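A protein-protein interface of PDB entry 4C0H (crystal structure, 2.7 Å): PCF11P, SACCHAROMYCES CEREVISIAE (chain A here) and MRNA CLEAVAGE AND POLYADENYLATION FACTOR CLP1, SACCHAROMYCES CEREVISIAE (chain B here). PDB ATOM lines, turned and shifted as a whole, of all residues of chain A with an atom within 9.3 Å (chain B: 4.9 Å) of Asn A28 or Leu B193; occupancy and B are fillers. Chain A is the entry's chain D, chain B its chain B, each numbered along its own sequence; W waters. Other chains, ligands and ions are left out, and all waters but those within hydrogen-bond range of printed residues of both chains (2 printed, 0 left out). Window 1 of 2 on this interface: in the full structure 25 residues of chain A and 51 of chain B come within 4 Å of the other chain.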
ATOM      1  N   GLN A  25      -6.687  24.933   9.290  1.00  0.00           N
ATOM      2  CA  GLN A  25      -5.362  24.686   9.829  1.00  0.00           C
ATOM      3  C   GLN A  25      -5.048  25.635  11.006  1.00  0.00           C
ATOM      4  O   GLN A  25      -5.781  26.593  11.253  1.00  0.00           O
ATOM      5  CB  GLN A  25      -4.272  24.611   8.765  1.00  0.00           C
ATOM      6  CG  GLN A  25      -4.079  25.909   8.003  1.00  0.00           C
ATOM      7  CD  GLN A  25      -2.888  25.878   7.122  1.00  0.00           C
ATOM      8  OE1 GLN A  25      -1.753  25.632   7.555  1.00  0.00           O
ATOM      9  NE2 GLN A  25      -3.129  26.152   5.873  1.00  0.00           N
ATOM     10  N   SER A  26      -3.994  25.331  11.759  1.00  0.00           N
ATOM     11  CA  SER A  26      -3.633  26.069  12.963  1.00  0.00           C
ATOM     12  C   SER A  26      -2.130  26.225  13.086  1.00  0.00           C
ATOM     13  O   SER A  26      -1.390  25.498  12.435  1.00  0.00           O
ATOM     14  CB  SER A  26      -4.152  25.322  14.199  1.00  0.00           C
ATOM     15  OG  SER A  26      -5.567  25.294  14.207  1.00  0.00           O
ATOM     16  N   ARG A  27      -1.690  27.139  13.970  1.00  0.00           N
ATOM     17  CA  ARG A  27      -0.288  27.351  14.322  1.00  0.00           C
ATOM     18  C   ARG A  27       0.103  26.118  15.138  1.00  0.00           C
ATOM     19  O   ARG A  27      -0.712  25.575  15.895  1.00  0.00           O
ATOM     20  CB  ARG A  27      -0.156  28.628  15.190  1.00  0.00           C
ATOM     21  CG  ARG A  27       1.247  29.031  15.672  1.00  0.00           C
ATOM     22  CD  ARG A  27       2.102  29.667  14.612  1.00  0.00           C
ATOM     23  NE  ARG A  27       1.457  30.832  14.014  1.00  0.00           N
ATOM     24  CZ  ARG A  27       1.520  31.157  12.729  1.00  0.00           C
ATOM     25  NH1 ARG A  27       2.191  30.392  11.873  1.00  0.00           N
ATOM     26  NH2 ARG A  27       0.884  32.229  12.280  1.00  0.00           N
ATOM     27  N   ASN A  28       1.330  25.647  14.947  1.00  0.00           N
ATOM     28  CA  ASN A  28       1.834  24.500  15.688  1.00  0.00           C
ATOM     29  C   ASN A  28       2.599  24.972  16.906  1.00  0.00           C
ATOM     30  O   ASN A  28       3.177  26.047  16.889  1.00  0.00           O
ATOM     31  CB  ASN A  28       2.772  23.666  14.817  1.00  0.00           C
ATOM     32  CG  ASN A  28       2.151  22.924  13.667  1.00  0.00           C
ATOM     33  OD1 ASN A  28       0.945  22.690  13.600  1.00  0.00           O
ATOM     34  ND2 ASN A  28       2.992  22.503  12.745  1.00  0.00           N
ATOM     35  N   TRP A  29       2.669  24.115  17.946  1.00  0.00           N
ATOM     36  CA  TRP A  29       3.512  24.365  19.122  1.00  0.00           C
ATOM     37  C   TRP A  29       4.987  24.287  18.669  1.00  0.00           C
ATOM     38  O   TRP A  29       5.302  23.688  17.625  1.00  0.00           O
ATOM     39  CB  TRP A  29       3.285  23.281  20.166  1.00  0.00           C
ATOM     40  CG  TRP A  29       1.914  23.211  20.767  1.00  0.00           C
ATOM     41  CD1 TRP A  29       1.086  22.124  20.778  1.00  0.00           C
ATOM     42  CD2 TRP A  29       1.269  24.212  21.587  1.00  0.00           C
ATOM     43  NE1 TRP A  29      -0.046  22.393  21.517  1.00  0.00           N
ATOM     44  CE2 TRP A  29       0.038  23.664  22.026  1.00  0.00           C
ATOM     45  CE3 TRP A  29       1.592  25.535  21.957  1.00  0.00           C
ATOM     46  CZ2 TRP A  29      -0.875  24.392  22.792  1.00  0.00           C
ATOM     47  CZ3 TRP A  29       0.699  26.243  22.748  1.00  0.00           C
ATOM     48  CH2 TRP A  29      -0.526  25.676  23.143  1.00  0.00           C
ATOM     49  N   TYR A  30       5.884  24.910  19.430  1.00  0.00           N
ATOM     50  CA  TYR A  30       7.330  24.863  19.126  1.00  0.00           C
ATOM     51  C   TYR A  30       7.880  23.514  19.612  1.00  0.00           C
ATOM     52  O   TYR A  30       7.242  22.853  20.443  1.00  0.00           O
ATOM     53  CB  TYR A  30       8.083  26.045  19.803  1.00  0.00           C
ATOM     54  CG  TYR A  30       7.614  27.420  19.364  1.00  0.00           C
ATOM     55  CD1 TYR A  30       7.481  27.733  18.014  1.00  0.00           C
ATOM     56  CD2 TYR A  30       7.280  28.403  20.298  1.00  0.00           C
ATOM     57  CE1 TYR A  30       7.027  28.981  17.599  1.00  0.00           C
ATOM     58  CE2 TYR A  30       6.815  29.661  19.891  1.00  0.00           C
ATOM     59  CZ  TYR A  30       6.666  29.933  18.536  1.00  0.00           C
ATOM     60  OH  TYR A  30       6.187  31.134  18.057  1.00  0.00           O
ATOM     61  N   LEU A  31       9.033  23.090  19.072  1.00  0.00           N
ATOM     62  CA  LEU A  31       9.740  21.875  19.521  1.00  0.00           C
ATOM     63  C   LEU A  31      10.558  22.193  20.776  1.00  0.00           C
ATOM     64  O   LEU A  31      10.911  23.351  21.019  1.00  0.00           O
ATOM     65  CB  LEU A  31      10.686  21.345  18.428  1.00  0.00           C
ATOM     66  CG  LEU A  31      10.073  20.900  17.092  1.00  0.00           C
ATOM     67  CD1 LEU A  31      11.143  20.401  16.154  1.00  0.00           C
ATOM     68  CD2 LEU A  31       9.017  19.864  17.277  1.00  0.00           C
ATOM     69  N   TRP A  36      14.325  20.206  18.590  1.00  0.00           N
ATOM     70  CA  TRP A  36      14.749  21.290  17.701  1.00  0.00           C
ATOM     71  C   TRP A  36      16.195  21.120  17.204  1.00  0.00           C
ATOM     72  O   TRP A  36      16.437  21.350  16.029  1.00  0.00           O
ATOM     73  CB  TRP A  36      14.536  22.672  18.352  1.00  0.00           C
ATOM     74  CG  TRP A  36      14.806  23.809  17.414  1.00  0.00           C
ATOM     75  CD1 TRP A  36      13.983  24.284  16.437  1.00  0.00           C
ATOM     76  CD2 TRP A  36      16.019  24.581  17.327  1.00  0.00           C
ATOM     77  NE1 TRP A  36      14.599  25.326  15.760  1.00  0.00           N
ATOM     78  CE2 TRP A  36      15.851  25.516  16.277  1.00  0.00           C
ATOM     79  CE3 TRP A  36      17.221  24.606  18.073  1.00  0.00           C
ATOM     80  CZ2 TRP A  36      16.854  26.422  15.912  1.00  0.00           C
ATOM     81  CZ3 TRP A  36      18.222  25.497  17.704  1.00  0.00           C
ATOM     82  CH2 TRP A  36      18.033  26.398  16.643  1.00  0.00           C
ATOM     83  N   PHE A  39      16.337  18.518  14.536  1.00  0.00           N
ATOM     84  CA  PHE A  39      15.489  18.811  13.378  1.00  0.00           C
ATOM     85  C   PHE A  39      16.294  19.286  12.177  1.00  0.00           C
ATOM     86  O   PHE A  39      17.271  20.031  12.309  1.00  0.00           O
ATOM     87  CB  PHE A  39      14.425  19.856  13.742  1.00  0.00           C
ATOM     88  CG  PHE A  39      13.311  20.047  12.728  1.00  0.00           C
ATOM     89  CD1 PHE A  39      12.190  19.203  12.724  1.00  0.00           C
ATOM     90  CD2 PHE A  39      13.365  21.090  11.783  1.00  0.00           C
ATOM     91  CE1 PHE A  39      11.147  19.397  11.786  1.00  0.00           C
ATOM     92  CE2 PHE A  39      12.329  21.275  10.843  1.00  0.00           C
ATOM     93  CZ  PHE A  39      11.219  20.438  10.860  1.00  0.00           C
ATOM     94  N   LYS A  40      15.846  18.859  10.976  1.00  0.00           N
ATOM     95  CA  LYS A  40      16.425  19.214   9.684  1.00  0.00           C
ATOM     96  C   LYS A  40      15.295  19.871   8.904  1.00  0.00           C
ATOM     97  O   LYS A  40      14.263  19.258   8.667  1.00  0.00           O
ATOM     98  CB  LYS A  40      16.950  17.964   8.939  1.00  0.00           C
ATOM     99  CG  LYS A  40      17.967  17.098   9.692  1.00  0.00           C
ATOM    100  CD  LYS A  40      19.334  17.731   9.842  1.00  0.00           C
ATOM    101  CE  LYS A  40      20.308  16.891  10.620  1.00  0.00           C
ATOM    102  NZ  LYS A  40      19.914  16.690  12.037  1.00  0.00           N
ATOM    103  N   ASP A  41      15.481  21.128   8.518  1.00  0.00           N
ATOM    104  CA  ASP A  41      14.494  21.895   7.776  1.00  0.00           C
ATOM    105  C   ASP A  41      14.154  21.315   6.411  1.00  0.00           C
ATOM    106  O   ASP A  41      13.174  21.748   5.822  1.00  0.00           O
ATOM    107  CB  ASP A  41      14.901  23.368   7.703  1.00  0.00           C
ATOM    108  CG  ASP A  41      14.547  24.180   8.934  1.00  0.00           C
ATOM    109  OD1 ASP A  41      14.701  23.648  10.072  1.00  0.00           O
ATOM    110  OD2 ASP A  41      14.100  25.345   8.770  1.00  0.00           O
ATOM    111  N   GLU A  43      12.900  18.549   6.051  1.00  0.00           N
ATOM    112  CA  GLU A  43      11.603  17.948   6.390  1.00  0.00           C
ATOM    113  C   GLU A  43      10.503  18.931   5.971  1.00  0.00           C
ATOM    114  O   GLU A  43       9.471  18.497   5.457  1.00  0.00           O
ATOM    115  CB  GLU A  43      11.476  17.688   7.896  1.00  0.00           C
ATOM    116  CG  GLU A  43      12.343  16.548   8.407  1.00  0.00           C
ATOM    117  CD  GLU A  43      12.334  16.345   9.915  1.00  0.00           C
ATOM    118  OE1 GLU A  43      11.242  16.052  10.461  1.00  0.00           O
ATOM    119  OE2 GLU A  43      13.418  16.451  10.543  1.00  0.00           O
ATOM    120  N   ILE A  44      10.722  20.255   6.179  1.00  0.00           N
ATOM    121  CA  ILE A  44       9.747  21.289   5.799  1.00  0.00           C
ATOM    122  C   ILE A  44       9.679  21.385   4.256  1.00  0.00           C
ATOM    123  O   ILE A  44       8.642  21.076   3.654  1.00  0.00           O
ATOM    124  CB  ILE A  44      10.022  22.693   6.445  1.00  0.00           C
ATOM    125  CG1 ILE A  44      10.207  22.625   7.982  1.00  0.00           C
ATOM    126  CG2 ILE A  44       8.951  23.716   6.010  1.00  0.00           C
ATOM    127  CD1 ILE A  44      10.852  23.857   8.626  1.00  0.00           C
ATOM    128  N   THR A  45      10.817  21.782   3.649  1.00  0.00           N
ATOM    129  CA  THR A  45      11.039  22.016   2.226  1.00  0.00           C
ATOM    130  C   THR A  45      11.070  20.724   1.356  1.00  0.00           C
ATOM    131  O   THR A  45      11.816  20.659   0.372  1.00  0.00           O
ATOM    132  CB  THR A  45      12.229  22.984   2.058  1.00  0.00           C
ATOM    133  OG1 THR A  45      13.406  22.345   2.524  1.00  0.00           O
ATOM    134  CG2 THR A  45      12.044  24.282   2.842  1.00  0.00           C
ATOM    135  N   GLN B 191       6.405  33.242   9.022  1.00  0.00           N
ATOM    136  CA  GLN B 191       5.707  32.547  10.121  1.00  0.00           C
ATOM    137  C   GLN B 191       6.283  31.216  10.502  1.00  0.00           C
ATOM    138  O   GLN B 191       6.954  30.580   9.699  1.00  0.00           O
ATOM    139  CB  GLN B 191       4.230  32.332   9.742  1.00  0.00           C
ATOM    140  CG  GLN B 191       3.505  33.609   9.405  1.00  0.00           C
ATOM    141  CD  GLN B 191       2.134  33.328   8.913  1.00  0.00           C
ATOM    142  OE1 GLN B 191       1.326  32.686   9.583  1.00  0.00           O
ATOM    143  NE2 GLN B 191       1.845  33.816   7.731  1.00  0.00           N
ATOM    144  N   SER B 192       5.963  30.761  11.716  1.00  0.00           N
ATOM    145  CA  SER B 192       6.359  29.444  12.195  1.00  0.00           C
ATOM    146  C   SER B 192       5.430  28.372  11.613  1.00  0.00           C
ATOM    147  O   SER B 192       4.427  28.720  11.017  1.00  0.00           O
ATOM    148  CB  SER B 192       6.486  29.391  13.720  1.00  0.00           C
ATOM    149  OG  SER B 192       5.458  30.021  14.461  1.00  0.00           O
ATOM    150  N   LEU B 193       5.789  27.078  11.730  1.00  0.00           N
ATOM    151  CA  LEU B 193       4.992  25.970  11.180  1.00  0.00           C
ATOM    152  C   LEU B 193       3.534  25.952  11.531  1.00  0.00           C
ATOM    153  O   LEU B 193       3.147  26.403  12.612  1.00  0.00           O
ATOM    154  CB  LEU B 193       5.624  24.592  11.457  1.00  0.00           C
ATOM    155  CG  LEU B 193       7.077  24.369  10.944  1.00  0.00           C
ATOM    156  CD1 LEU B 193       7.487  22.936  11.108  1.00  0.00           C
ATOM    157  CD2 LEU B 193       7.256  24.791   9.478  1.00  0.00           C
ATOM    158  N   THR B 194       2.721  25.454  10.576  1.00  0.00           N
ATOM    159  CA  THR B 194       1.279  25.297  10.700  1.00  0.00           C
ATOM    160  C   THR B 194       0.890  23.831  10.401  1.00  0.00           C
ATOM    161  O   THR B 194       1.638  23.101   9.743  1.00  0.00           O
ATOM    162  CB  THR B 194       0.531  26.263   9.768  1.00  0.00           C
ATOM    163  OG1 THR B 194       0.833  25.913   8.418  1.00  0.00           O
ATOM    164  CG2 THR B 194       0.827  27.728  10.048  1.00  0.00           C
ATOM    165  N   SER B 195      -0.312  23.434  10.829  1.00  0.00           N
ATOM    166  CA  SER B 195      -0.830  22.081  10.692  1.00  0.00           C
ATOM    167  C   SER B 195      -1.273  21.710   9.267  1.00  0.00           C
ATOM    168  O   SER B 195      -1.646  20.556   9.009  1.00  0.00           O
ATOM    169  CB  SER B 195      -1.986  21.893  11.666  1.00  0.00           C
ATOM    170  OG  SER B 195      -3.054  22.777  11.369  1.00  0.00           O
ATOM    171  N   ASN B 202       7.095  27.558   5.773  1.00  0.00           N
ATOM    172  CA  ASN B 202       7.200  28.310   7.014  1.00  0.00           C
ATOM    173  C   ASN B 202       8.460  27.909   7.765  1.00  0.00           C
ATOM    174  O   ASN B 202       9.152  26.942   7.401  1.00  0.00           O
ATOM    175  CB  ASN B 202       5.954  28.093   7.865  1.00  0.00           C
ATOM    176  CG  ASN B 202       4.691  28.657   7.266  1.00  0.00           C
ATOM    177  OD1 ASN B 202       4.698  29.639   6.524  1.00  0.00           O
ATOM    178  ND2 ASN B 202       3.567  28.074   7.626  1.00  0.00           N
ATOM    179  N   LYS B 203       8.740  28.661   8.825  1.00  0.00           N
ATOM    180  CA  LYS B 203       9.888  28.508   9.677  1.00  0.00           C
ATOM    181  C   LYS B 203       9.660  27.693  10.944  1.00  0.00           C
ATOM    182  O   LYS B 203       8.521  27.499  11.365  1.00  0.00           O
ATOM    183  CB  LYS B 203      10.445  29.892   9.959  1.00  0.00           C
ATOM    184  CG  LYS B 203      11.550  30.269   8.970  1.00  0.00           C
ATOM    185  CD  LYS B 203      11.039  30.656   7.611  1.00  0.00           C
ATOM    186  CE  LYS B 203      12.139  30.720   6.609  1.00  0.00           C
ATOM    187  NZ  LYS B 203      11.585  30.440   5.276  1.00  0.00           N
ATOM    188  N   GLN B 204      10.735  27.137  11.505  1.00  0.00           N
ATOM    189  CA  GLN B 204      10.708  26.336  12.723  1.00  0.00           C
ATOM    190  C   GLN B 204      11.690  27.021  13.711  1.00  0.00           C
ATOM    191  O   GLN B 204      12.888  26.667  13.787  1.00  0.00           O
ATOM    192  CB  GLN B 204      11.090  24.861  12.421  1.00  0.00           C
ATOM    193  CG  GLN B 204      11.233  23.958  13.641  1.00  0.00           C
ATOM    194  CD  GLN B 204       9.915  23.466  14.161  1.00  0.00           C
ATOM    195  OE1 GLN B 204       9.247  24.115  14.972  1.00  0.00           O
ATOM    196  NE2 GLN B 204       9.525  22.296  13.724  1.00  0.00           N
ATOM    197  N   VAL B 427      -3.280  26.189  19.110  1.00  0.00           N
ATOM    198  CA  VAL B 427      -3.534  24.789  18.756  1.00  0.00           C
ATOM    199  C   VAL B 427      -4.861  24.309  19.302  1.00  0.00           C
ATOM    200  O   VAL B 427      -5.049  24.371  20.515  1.00  0.00           O
ATOM    201  CB  VAL B 427      -2.345  23.895  19.238  1.00  0.00           C
ATOM    202  CG1 VAL B 427      -2.510  22.455  18.791  1.00  0.00           C
ATOM    203  CG2 VAL B 427      -0.997  24.461  18.759  1.00  0.00           C
HETATM  204  O   HOH W   1      10.365  24.965  17.274  1.00  0.00           O
HETATM  205  O   HOH W   2      13.243  27.380  10.251  1.00  0.00           O
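Water W2 bridges OD2 of Asp A41 (2.7 Å) and N of Gln B204 (2.8 Å).
Water W1 lies within hydrogen-bond range of the side-chain amide oxygen (OE1) of Gln B204 and the backbone NH (N) of Leu A31.
Of chain B, only Leu B193, Thr B194 and Ser B195 come within 4 Å of Asn A28.
Of chain A, only Arg A27 (3.95 Å), Asn A28 (3.1 Å) and Ile A44 (3.8 Å) come within 4 Å of Leu B193.
Of the printed residues of chain A, Thr B194 touches Gln A25 (2.7 Å), Ser A26 (3.2 Å), Arg A27 (3.5 Å) and Asn A28 (3.3 Å).
Of the printed residues of chain A, Gln B191 touches Arg A27 (2.8 Å).
Printed residues of chain B within 4 Å of Ser A26: Thr B194 (3.2 Å) and Ser B195 (2.7 Å).
Of the printed residues of chain B, Leu A31 touches Gln B204 (3.5 Å).
Of the printed residues of chain B, Gln A25 touches Thr B194 (2.7 Å) and Ser B195 (3.4 Å).
The nearest residue of chain B that does not touch Asn A28 is Val B427 (4.1 Å).
The nearest residue of chain A that does not touch Leu B193 is Phe A39 (4.5 Å).
The backbone carbonyl oxygen of Gln B191 sits at hydrogen-bond distance from the backbone NH of Lys B203, 2.8 Å away.
The backbone NH (N) of Leu B193 lies within hydrogen-bond range of the backbone carbonyl oxygen (O) of Lys B203 (2.8 Å).
Printed residues of chain B that touch a printed residue of chain A: Gln B191, Ser B192, Leu B193, Thr B194, Ser B195, Asn B202, Gln B204 and Val B427.
Along chain B the printed residues that touch a printed residue of chain A span positions 191 to 427.
Hydrophobic or aromatic side chains of chain A that line the printed part of chain B: Trp A29, Tyr A30, Leu A31, Trp A36, Phe A39 and Ile A44.
Among the printed residues, 20 pairs touch across the chains.
Among the printed residues, pairs that only touch across the chains: Gln A25 with Ser B195 (3.4 Å), Ser A26 with Thr B194 (3.2 Å), Arg A27 with Leu B193 (3.95 Å), Arg A27 with Thr B194 (3.5 Å), Arg A27 with Val B427 (3.1 Å), Trp A29 with Val B427 (3.5 Å), Tyr A30 with Ser B192 (3.7 Å), Leu A31 with Gln B204 (3.5 Å), Phe A39 with Gln B204 (3.8 Å), Ile A44 with Leu B193 (3.8 Å), Ile A44 with Asn B202 (3.5 Å) and Ile A44 with Gln B204 (3.9 Å).
OE1 of Gln B191 is in hydrogen-bond range of NH2 of Arg A27 (2.8 Å).
The backbone carbonyl oxygen of Ser B192 lies within hydrogen-bond range of the guanidinium group of Arg A27 (2.9 Å).
The backbone NH (N) of Asn A28 lies within hydrogen-bond range of the backbone carbonyl oxygen (O) of Leu B193 (3.1 Å).
The side-chain amide oxygen of Gln A25 lies within hydrogen-bond range of the side-chain hydroxyl of Thr B194 (2.7 Å).
The backbone carbonyl oxygen (O) of Thr B194 lies within hydrogen-bond range of the side-chain amide nitrogen (ND2) of Asn A28 (3.3 Å).
The backbone NH of Ser A26 lies within hydrogen-bond range of the side-chain hydroxyl of Ser B195 (2.7 Å).
OD1 of Asn A28 is in hydrogen-bond range of N of Ser B195.
NE1 of Trp A36 is in hydrogen-bond range of O of Gln B204, 2.9 Å away.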
